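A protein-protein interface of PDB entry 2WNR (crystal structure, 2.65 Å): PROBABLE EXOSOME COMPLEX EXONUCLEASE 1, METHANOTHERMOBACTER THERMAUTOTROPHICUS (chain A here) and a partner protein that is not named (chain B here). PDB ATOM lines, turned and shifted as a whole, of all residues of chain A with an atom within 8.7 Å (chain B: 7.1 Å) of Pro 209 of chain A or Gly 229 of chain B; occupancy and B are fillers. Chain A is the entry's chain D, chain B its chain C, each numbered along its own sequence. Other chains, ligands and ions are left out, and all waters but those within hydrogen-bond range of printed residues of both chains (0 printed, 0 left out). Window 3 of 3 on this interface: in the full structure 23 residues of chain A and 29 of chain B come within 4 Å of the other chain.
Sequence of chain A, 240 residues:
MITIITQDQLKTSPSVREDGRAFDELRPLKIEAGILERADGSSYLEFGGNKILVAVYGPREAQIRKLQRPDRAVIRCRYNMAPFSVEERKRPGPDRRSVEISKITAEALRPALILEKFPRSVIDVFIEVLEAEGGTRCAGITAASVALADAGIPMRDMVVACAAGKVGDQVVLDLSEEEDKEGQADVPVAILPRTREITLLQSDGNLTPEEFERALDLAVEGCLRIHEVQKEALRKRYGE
N of Ile 231 of chain B sits at hydrogen-bond distance from O of Leu 207 of chain A (2.6 Å). The side-chain hydroxyl of Ser 230 of chain B lies within hydrogen-bond range of the side-chain amide oxygen of Asn 206 of chain A, 2.9 Å away.
OG1 of Thr 226 of chain B lies within hydrogen-bond range of OG of Ser 230 of chain B (2.8 Å). O of Leu 248 of chain B is in hydrogen-bond range of OG of Ser 252 of chain B.
O of Ile 231 of chain B touches CA of Asn 206 of chain A, at 3.6 Å. O of Leu 207 of chain A touches CA of Ser 230 of chain B, 3.4 Å away. Pro 209 of chain A touches Gly 229 of chain B (CD to O, 3.6 Å). CB of Pro 209 of chain A touches CG1 of Val 251 of chain B, 3.9 Å away. CG of Pro 209 of chain A touches CG2 of Val 255 of chain B (3.8 Å). Ile 231 of chain B touches Phe 212 of chain A. Leu 248 of chain B touches Glu 213 of chain A.
Of chain B, only Gly 229, Val 251 and Val 255 come within 4 Å of Pro 209 of chain A. Of chain A, only Pro 209 (3.6 Å) comes within 4 Å of Gly 229 of chain B. Ser 230 of chain B touches just these residues of chain A: Asn 206 (2.9 Å) and Leu 207 (3.4 Å). Printed residues of chain A within 4 Å of Ile 231 of chain B: Asn 206 (3.6 Å), Leu 207 (2.6 Å) and Phe 212 (3.99 Å). Of the printed residues of chain B, Glu 213 of chain A touches Leu 248. The nearest printed residue of chain A that does not touch Val 255 of chain B is Thr 208 of chain A (7.0 Å).
Printed residues of chain B that touch a printed residue of chain A: Gly 229, Ser 230, Ile 231, Leu 248, Val 251 and Val 255. Hydrophobic or aromatic side chains of chain B within 4 Å of the printed part of chain A: Ile 231, Leu 248, Val 251 and Val 255. Along chain B the printed residues that touch a printed residue of chain A span positions 229 to 255. Of the 11 printed residues of chain A, 5 touch a printed residue of chain B. Hydrophobic or aromatic side chains of chain A that line the printed part of chain B: Pro 209 and Phe 212. Among the printed residues, no Asp or Glu carboxylate lies within 4 Å of a Lys or Arg side-chain nitrogen of the other chain.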
ATOM      1  N   ASN A 206      23.724   6.016  19.152  1.00  0.00           N
ATOM      2  CA  ASN A 206      23.567   7.387  19.642  1.00  0.00           C
ATOM      3  C   ASN A 206      24.194   7.623  21.015  1.00  0.00           C
ATOM      4  O   ASN A 206      23.650   7.208  22.046  1.00  0.00           O
ATOM      5  CB  ASN A 206      22.092   7.778  19.660  1.00  0.00           C
ATOM      6  CG  ASN A 206      21.897   9.270  19.688  1.00  0.00           C
ATOM      7  OD1 ASN A 206      22.230   9.963  18.724  1.00  0.00           O
ATOM      8  ND2 ASN A 206      21.350   9.781  20.789  1.00  0.00           N
ATOM      9  N   LEU A 207      25.337   8.298  21.019  1.00  0.00           N
ATOM     10  CA  LEU A 207      26.061   8.591  22.251  1.00  0.00           C
ATOM     11  C   LEU A 207      26.300  10.094  22.420  1.00  0.00           C
ATOM     12  O   LEU A 207      26.579  10.800  21.450  1.00  0.00           O
ATOM     13  CB  LEU A 207      27.411   7.877  22.248  1.00  0.00           C
ATOM     14  CG  LEU A 207      27.483   6.352  22.296  1.00  0.00           C
ATOM     15  CD1 LEU A 207      28.867   5.894  21.904  1.00  0.00           C
ATOM     16  CD2 LEU A 207      27.135   5.827  23.673  1.00  0.00           C
ATOM     17  N   THR A 208      26.191  10.586  23.647  1.00  0.00           N
ATOM     18  CA  THR A 208      26.671  11.929  23.953  1.00  0.00           C
ATOM     19  C   THR A 208      28.193  11.845  24.093  1.00  0.00           C
ATOM     20  O   THR A 208      28.719  10.772  24.391  1.00  0.00           O
ATOM     21  CB  THR A 208      26.057  12.495  25.253  1.00  0.00           C
ATOM     22  OG1 THR A 208      26.444  11.678  26.365  1.00  0.00           O
ATOM     23  CG2 THR A 208      24.534  12.558  25.164  1.00  0.00           C
ATOM     24  N   PRO A 209      28.910  12.962  23.872  1.00  0.00           N
ATOM     25  CA  PRO A 209      30.376  12.942  23.965  1.00  0.00           C
ATOM     26  C   PRO A 209      30.844  12.425  25.312  1.00  0.00           C
ATOM     27  O   PRO A 209      31.931  11.844  25.420  1.00  0.00           O
ATOM     28  CB  PRO A 209      30.751  14.417  23.830  1.00  0.00           C
ATOM     29  CG  PRO A 209      29.639  15.010  23.050  1.00  0.00           C
ATOM     30  CD  PRO A 209      28.405  14.292  23.487  1.00  0.00           C
ATOM     31  N   GLU A 210      30.009  12.649  26.322  1.00  0.00           N
ATOM     32  CA  GLU A 210      30.249  12.188  27.680  1.00  0.00           C
ATOM     33  C   GLU A 210      30.050  10.674  27.757  1.00  0.00           C
ATOM     34  O   GLU A 210      30.883   9.973  28.330  1.00  0.00           O
ATOM     35  CB  GLU A 210      29.320  12.939  28.646  1.00  0.00           C
ATOM     36  CG  GLU A 210      29.589  12.713  30.135  1.00  0.00           C
ATOM     37  CD  GLU A 210      28.843  11.507  30.707  1.00  0.00           C
ATOM     38  OE1 GLU A 210      27.968  10.948  30.005  1.00  0.00           O
ATOM     39  OE2 GLU A 210      29.135  11.120  31.862  1.00  0.00           O
ATOM     40  N   GLU A 211      28.957  10.176  27.173  1.00  0.00           N
ATOM     41  CA  GLU A 211      28.686   8.735  27.128  1.00  0.00           C
ATOM     42  C   GLU A 211      29.774   7.997  26.372  1.00  0.00           C
ATOM     43  O   GLU A 211      30.218   6.929  26.793  1.00  0.00           O
ATOM     44  CB  GLU A 211      27.342   8.446  26.465  1.00  0.00           C
ATOM     45  CG  GLU A 211      26.131   8.656  27.352  1.00  0.00           C
ATOM     46  CD  GLU A 211      24.823   8.533  26.586  1.00  0.00           C
ATOM     47  OE1 GLU A 211      24.724   9.058  25.451  1.00  0.00           O
ATOM     48  OE2 GLU A 211      23.885   7.916  27.125  1.00  0.00           O
ATOM     49  N   PHE A 212      30.196   8.575  25.251  1.00  0.00           N
ATOM     50  CA  PHE A 212      31.228   7.974  24.429  1.00  0.00           C
ATOM     51  C   PHE A 212      32.528   7.828  25.209  1.00  0.00           C
ATOM     52  O   PHE A 212      33.131   6.761  25.212  1.00  0.00           O
ATOM     53  CB  PHE A 212      31.456   8.779  23.147  1.00  0.00           C
ATOM     54  CG  PHE A 212      32.651   8.322  22.365  1.00  0.00           C
ATOM     55  CD1 PHE A 212      32.556   7.246  21.491  1.00  0.00           C
ATOM     56  CD2 PHE A 212      33.885   8.949  22.528  1.00  0.00           C
ATOM     57  CE1 PHE A 212      33.663   6.812  20.787  1.00  0.00           C
ATOM     58  CE2 PHE A 212      35.002   8.515  21.825  1.00  0.00           C
ATOM     59  CZ  PHE A 212      34.891   7.449  20.956  1.00  0.00           C
ATOM     60  N   GLU A 213      32.948   8.904  25.871  1.00  0.00           N
ATOM     61  CA  GLU A 213      34.166   8.888  26.678  1.00  0.00           C
ATOM     62  C   GLU A 213      34.182   7.731  27.670  1.00  0.00           C
ATOM     63  O   GLU A 213      35.204   7.067  27.828  1.00  0.00           O
ATOM     64  CB  GLU A 213      34.344  10.216  27.411  1.00  0.00           C
ATOM     65  CG  GLU A 213      35.716  10.400  28.046  1.00  0.00           C
ATOM     66  CD  GLU A 213      35.925  11.801  28.602  1.00  0.00           C
ATOM     67  OE1 GLU A 213      35.437  12.769  27.982  1.00  0.00           O
ATOM     68  OE2 GLU A 213      36.585  11.940  29.652  1.00  0.00           O
ATOM     69  N   ARG A 214      33.056   7.489  28.332  1.00  0.00           N
ATOM     70  CA  ARG A 214      32.940   6.339  29.226  1.00  0.00           C
ATOM     71  C   ARG A 214      33.069   4.995  28.490  1.00  0.00           C
ATOM     72  O   ARG A 214      33.824   4.126  28.924  1.00  0.00           O
ATOM     73  CB  ARG A 214      31.640   6.401  30.031  1.00  0.00           C
ATOM     74  CG  ARG A 214      31.799   7.052  31.418  1.00  0.00           C
ATOM     75  CD  ARG A 214      30.448   7.508  31.955  1.00  0.00           C
ATOM     76  NE  ARG A 214      29.445   6.439  31.892  1.00  0.00           N
ATOM     77  CZ  ARG A 214      28.139   6.635  31.706  1.00  0.00           C
ATOM     78  NH1 ARG A 214      27.655   7.867  31.557  1.00  0.00           N
ATOM     79  NH2 ARG A 214      27.314   5.591  31.662  1.00  0.00           N
ATOM     80  N   ALA A 215      32.359   4.841  27.371  1.00  0.00           N
ATOM     81  CA  ALA A 215      32.350   3.574  26.624  1.00  0.00           C
ATOM     82  C   ALA A 215      33.709   3.191  26.049  1.00  0.00           C
ATOM     83  O   ALA A 215      34.105   2.024  26.102  1.00  0.00           O
ATOM     84  CB  ALA A 215      31.298   3.600  25.533  1.00  0.00           C
ATOM     85  N   LEU A 216      34.415   4.173  25.501  1.00  0.00           N
ATOM     86  CA  LEU A 216      35.807   4.000  25.101  1.00  0.00           C
ATOM     87  C   LEU A 216      36.668   3.510  26.279  1.00  0.00           C
ATOM     88  O   LEU A 216      37.338   2.476  26.161  1.00  0.00           O
ATOM     89  CB  LEU A 216      36.363   5.306  24.521  1.00  0.00           C
ATOM     90  CG  LEU A 216      37.874   5.491  24.344  1.00  0.00           C
ATOM     91  CD1 LEU A 216      38.398   4.641  23.208  1.00  0.00           C
ATOM     92  CD2 LEU A 216      38.217   6.944  24.106  1.00  0.00           C
ATOM     93  N   VAL B 225      28.165  13.783  13.837  1.00  0.00           N
ATOM     94  CA  VAL B 225      27.429  14.397  14.942  1.00  0.00           C
ATOM     95  C   VAL B 225      26.032  14.808  14.476  1.00  0.00           C
ATOM     96  O   VAL B 225      25.846  15.176  13.317  1.00  0.00           O
ATOM     97  CB  VAL B 225      28.172  15.629  15.498  1.00  0.00           C
ATOM     98  CG1 VAL B 225      27.540  16.092  16.780  1.00  0.00           C
ATOM     99  CG2 VAL B 225      29.637  15.314  15.732  1.00  0.00           C
ATOM    100  N   THR B 226      25.056  14.737  15.376  1.00  0.00           N
ATOM    101  CA  THR B 226      23.682  15.118  15.055  1.00  0.00           C
ATOM    102  C   THR B 226      23.394  16.572  15.436  1.00  0.00           C
ATOM    103  O   THR B 226      24.244  17.248  16.025  1.00  0.00           O
ATOM    104  CB  THR B 226      22.660  14.187  15.747  1.00  0.00           C
ATOM    105  OG1 THR B 226      22.696  14.383  17.172  1.00  0.00           O
ATOM    106  CG2 THR B 226      22.955  12.740  15.419  1.00  0.00           C
ATOM    107  N   GLU B 227      22.189  17.039  15.097  1.00  0.00           N
ATOM    108  CA  GLU B 227      21.733  18.394  15.434  1.00  0.00           C
ATOM    109  C   GLU B 227      21.891  18.730  16.909  1.00  0.00           C
ATOM    110  O   GLU B 227      22.338  19.821  17.245  1.00  0.00           O
ATOM    111  CB  GLU B 227      20.268  18.586  15.049  1.00  0.00           C
ATOM    112  CG  GLU B 227      20.025  18.794  13.565  1.00  0.00           C
ATOM    113  CD  GLU B 227      18.584  19.187  13.253  1.00  0.00           C
ATOM    114  OE1 GLU B 227      17.686  18.951  14.098  1.00  0.00           O
ATOM    115  OE2 GLU B 227      18.353  19.740  12.154  1.00  0.00           O
ATOM    116  N   GLU B 228      21.516  17.790  17.776  1.00  0.00           N
ATOM    117  CA  GLU B 228      21.551  17.994  19.233  1.00  0.00           C
ATOM    118  C   GLU B 228      22.891  17.602  19.881  1.00  0.00           C
ATOM    119  O   GLU B 228      22.961  17.362  21.086  1.00  0.00           O
ATOM    120  CB  GLU B 228      20.357  17.304  19.925  1.00  0.00           C
ATOM    121  CG  GLU B 228      20.047  15.878  19.457  1.00  0.00           C
ATOM    122  CD  GLU B 228      19.200  15.826  18.174  1.00  0.00           C
ATOM    123  OE1 GLU B 228      18.091  16.406  18.168  1.00  0.00           O
ATOM    124  OE2 GLU B 228      19.639  15.192  17.184  1.00  0.00           O
ATOM    125  N   GLY B 229      23.944  17.545  19.065  1.00  0.00           N
ATOM    126  CA  GLY B 229      25.311  17.361  19.542  1.00  0.00           C
ATOM    127  C   GLY B 229      25.694  15.971  20.022  1.00  0.00           C
ATOM    128  O   GLY B 229      26.636  15.825  20.793  1.00  0.00           O
ATOM    129  N   SER B 230      24.975  14.949  19.570  1.00  0.00           N
ATOM    130  CA  SER B 230      25.301  13.569  19.933  1.00  0.00           C
ATOM    131  C   SER B 230      25.989  12.840  18.779  1.00  0.00           C
ATOM    132  O   SER B 230      25.740  13.143  17.607  1.00  0.00           O
ATOM    133  CB  SER B 230      24.046  12.816  20.369  1.00  0.00           C
ATOM    134  OG  SER B 230      23.141  12.675  19.292  1.00  0.00           O
ATOM    135  N   ILE B 231      26.855  11.886  19.124  1.00  0.00           N
ATOM    136  CA  ILE B 231      27.661  11.149  18.142  1.00  0.00           C
ATOM    137  C   ILE B 231      26.889   9.962  17.554  1.00  0.00           C
ATOM    138  O   ILE B 231      26.482   9.053  18.280  1.00  0.00           O
ATOM    139  CB  ILE B 231      28.993  10.659  18.757  1.00  0.00           C
ATOM    140  CG1 ILE B 231      29.830  11.841  19.238  1.00  0.00           C
ATOM    141  CG2 ILE B 231      29.793   9.839  17.744  1.00  0.00           C
ATOM    142  CD1 ILE B 231      30.903  11.453  20.239  1.00  0.00           C
ATOM    143  N   LEU B 248      39.401  12.133  21.734  1.00  0.00           N
ATOM    144  CA  LEU B 248      38.526  13.025  22.489  1.00  0.00           C
ATOM    145  C   LEU B 248      38.615  14.464  22.002  1.00  0.00           C
ATOM    146  O   LEU B 248      37.637  15.210  22.071  1.00  0.00           O
ATOM    147  CB  LEU B 248      38.811  12.942  23.987  1.00  0.00           C
ATOM    148  CG  LEU B 248      38.560  11.599  24.674  1.00  0.00           C
ATOM    149  CD1 LEU B 248      38.878  11.722  26.152  1.00  0.00           C
ATOM    150  CD2 LEU B 248      37.132  11.099  24.475  1.00  0.00           C
ATOM    151  N   VAL B 251      36.446  14.546  18.817  1.00  0.00           N
ATOM    152  CA  VAL B 251      35.036  14.654  19.212  1.00  0.00           C
ATOM    153  C   VAL B 251      34.682  16.122  19.504  1.00  0.00           C
ATOM    154  O   VAL B 251      33.727  16.663  18.936  1.00  0.00           O
ATOM    155  CB  VAL B 251      34.704  13.755  20.442  1.00  0.00           C
ATOM    156  CG1 VAL B 251      33.277  13.999  20.929  1.00  0.00           C
ATOM    157  CG2 VAL B 251      34.921  12.279  20.120  1.00  0.00           C
ATOM    158  N   SER B 252      35.485  16.760  20.355  1.00  0.00           N
ATOM    159  CA  SER B 252      35.264  18.145  20.772  1.00  0.00           C
ATOM    160  C   SER B 252      35.093  19.119  19.611  1.00  0.00           C
ATOM    161  O   SER B 252      34.211  19.982  19.658  1.00  0.00           O
ATOM    162  CB  SER B 252      36.392  18.616  21.681  1.00  0.00           C
ATOM    163  OG  SER B 252      36.634  17.652  22.681  1.00  0.00           O
ATOM    164  N   VAL B 255      31.662  18.109  17.465  1.00  0.00           N
ATOM    165  CA  VAL B 255      30.517  18.698  18.172  1.00  0.00           C
ATOM    166  C   VAL B 255      30.429  20.205  17.915  1.00  0.00           C
ATOM    167  O   VAL B 255      29.341  20.742  17.696  1.00  0.00           O
ATOM    168  CB  VAL B 255      30.575  18.418  19.696  1.00  0.00           C
ATOM    169  CG1 VAL B 255      29.361  19.008  20.405  1.00  0.00           C
ATOM    170  CG2 VAL B 255      30.667  16.914  19.958  1.00  0.00           C
ATOM    171  N   PRO B 259      27.375  21.926  13.816  1.00  0.00           N
ATOM    172  CA  PRO B 259      26.357  22.977  13.760  1.00  0.00           C
ATOM    173  C   PRO B 259      26.648  24.065  12.711  1.00  0.00           C
ATOM    174  O   PRO B 259      25.714  24.588  12.090  1.00  0.00           O
ATOM    175  CB  PRO B 259      26.410  23.571  15.167  1.00  0.00           C
ATOM    176  CG  PRO B 259      26.780  22.434  16.018  1.00  0.00           C
ATOM    177  CD  PRO B 259      27.765  21.635  15.209  1.00  0.00           C
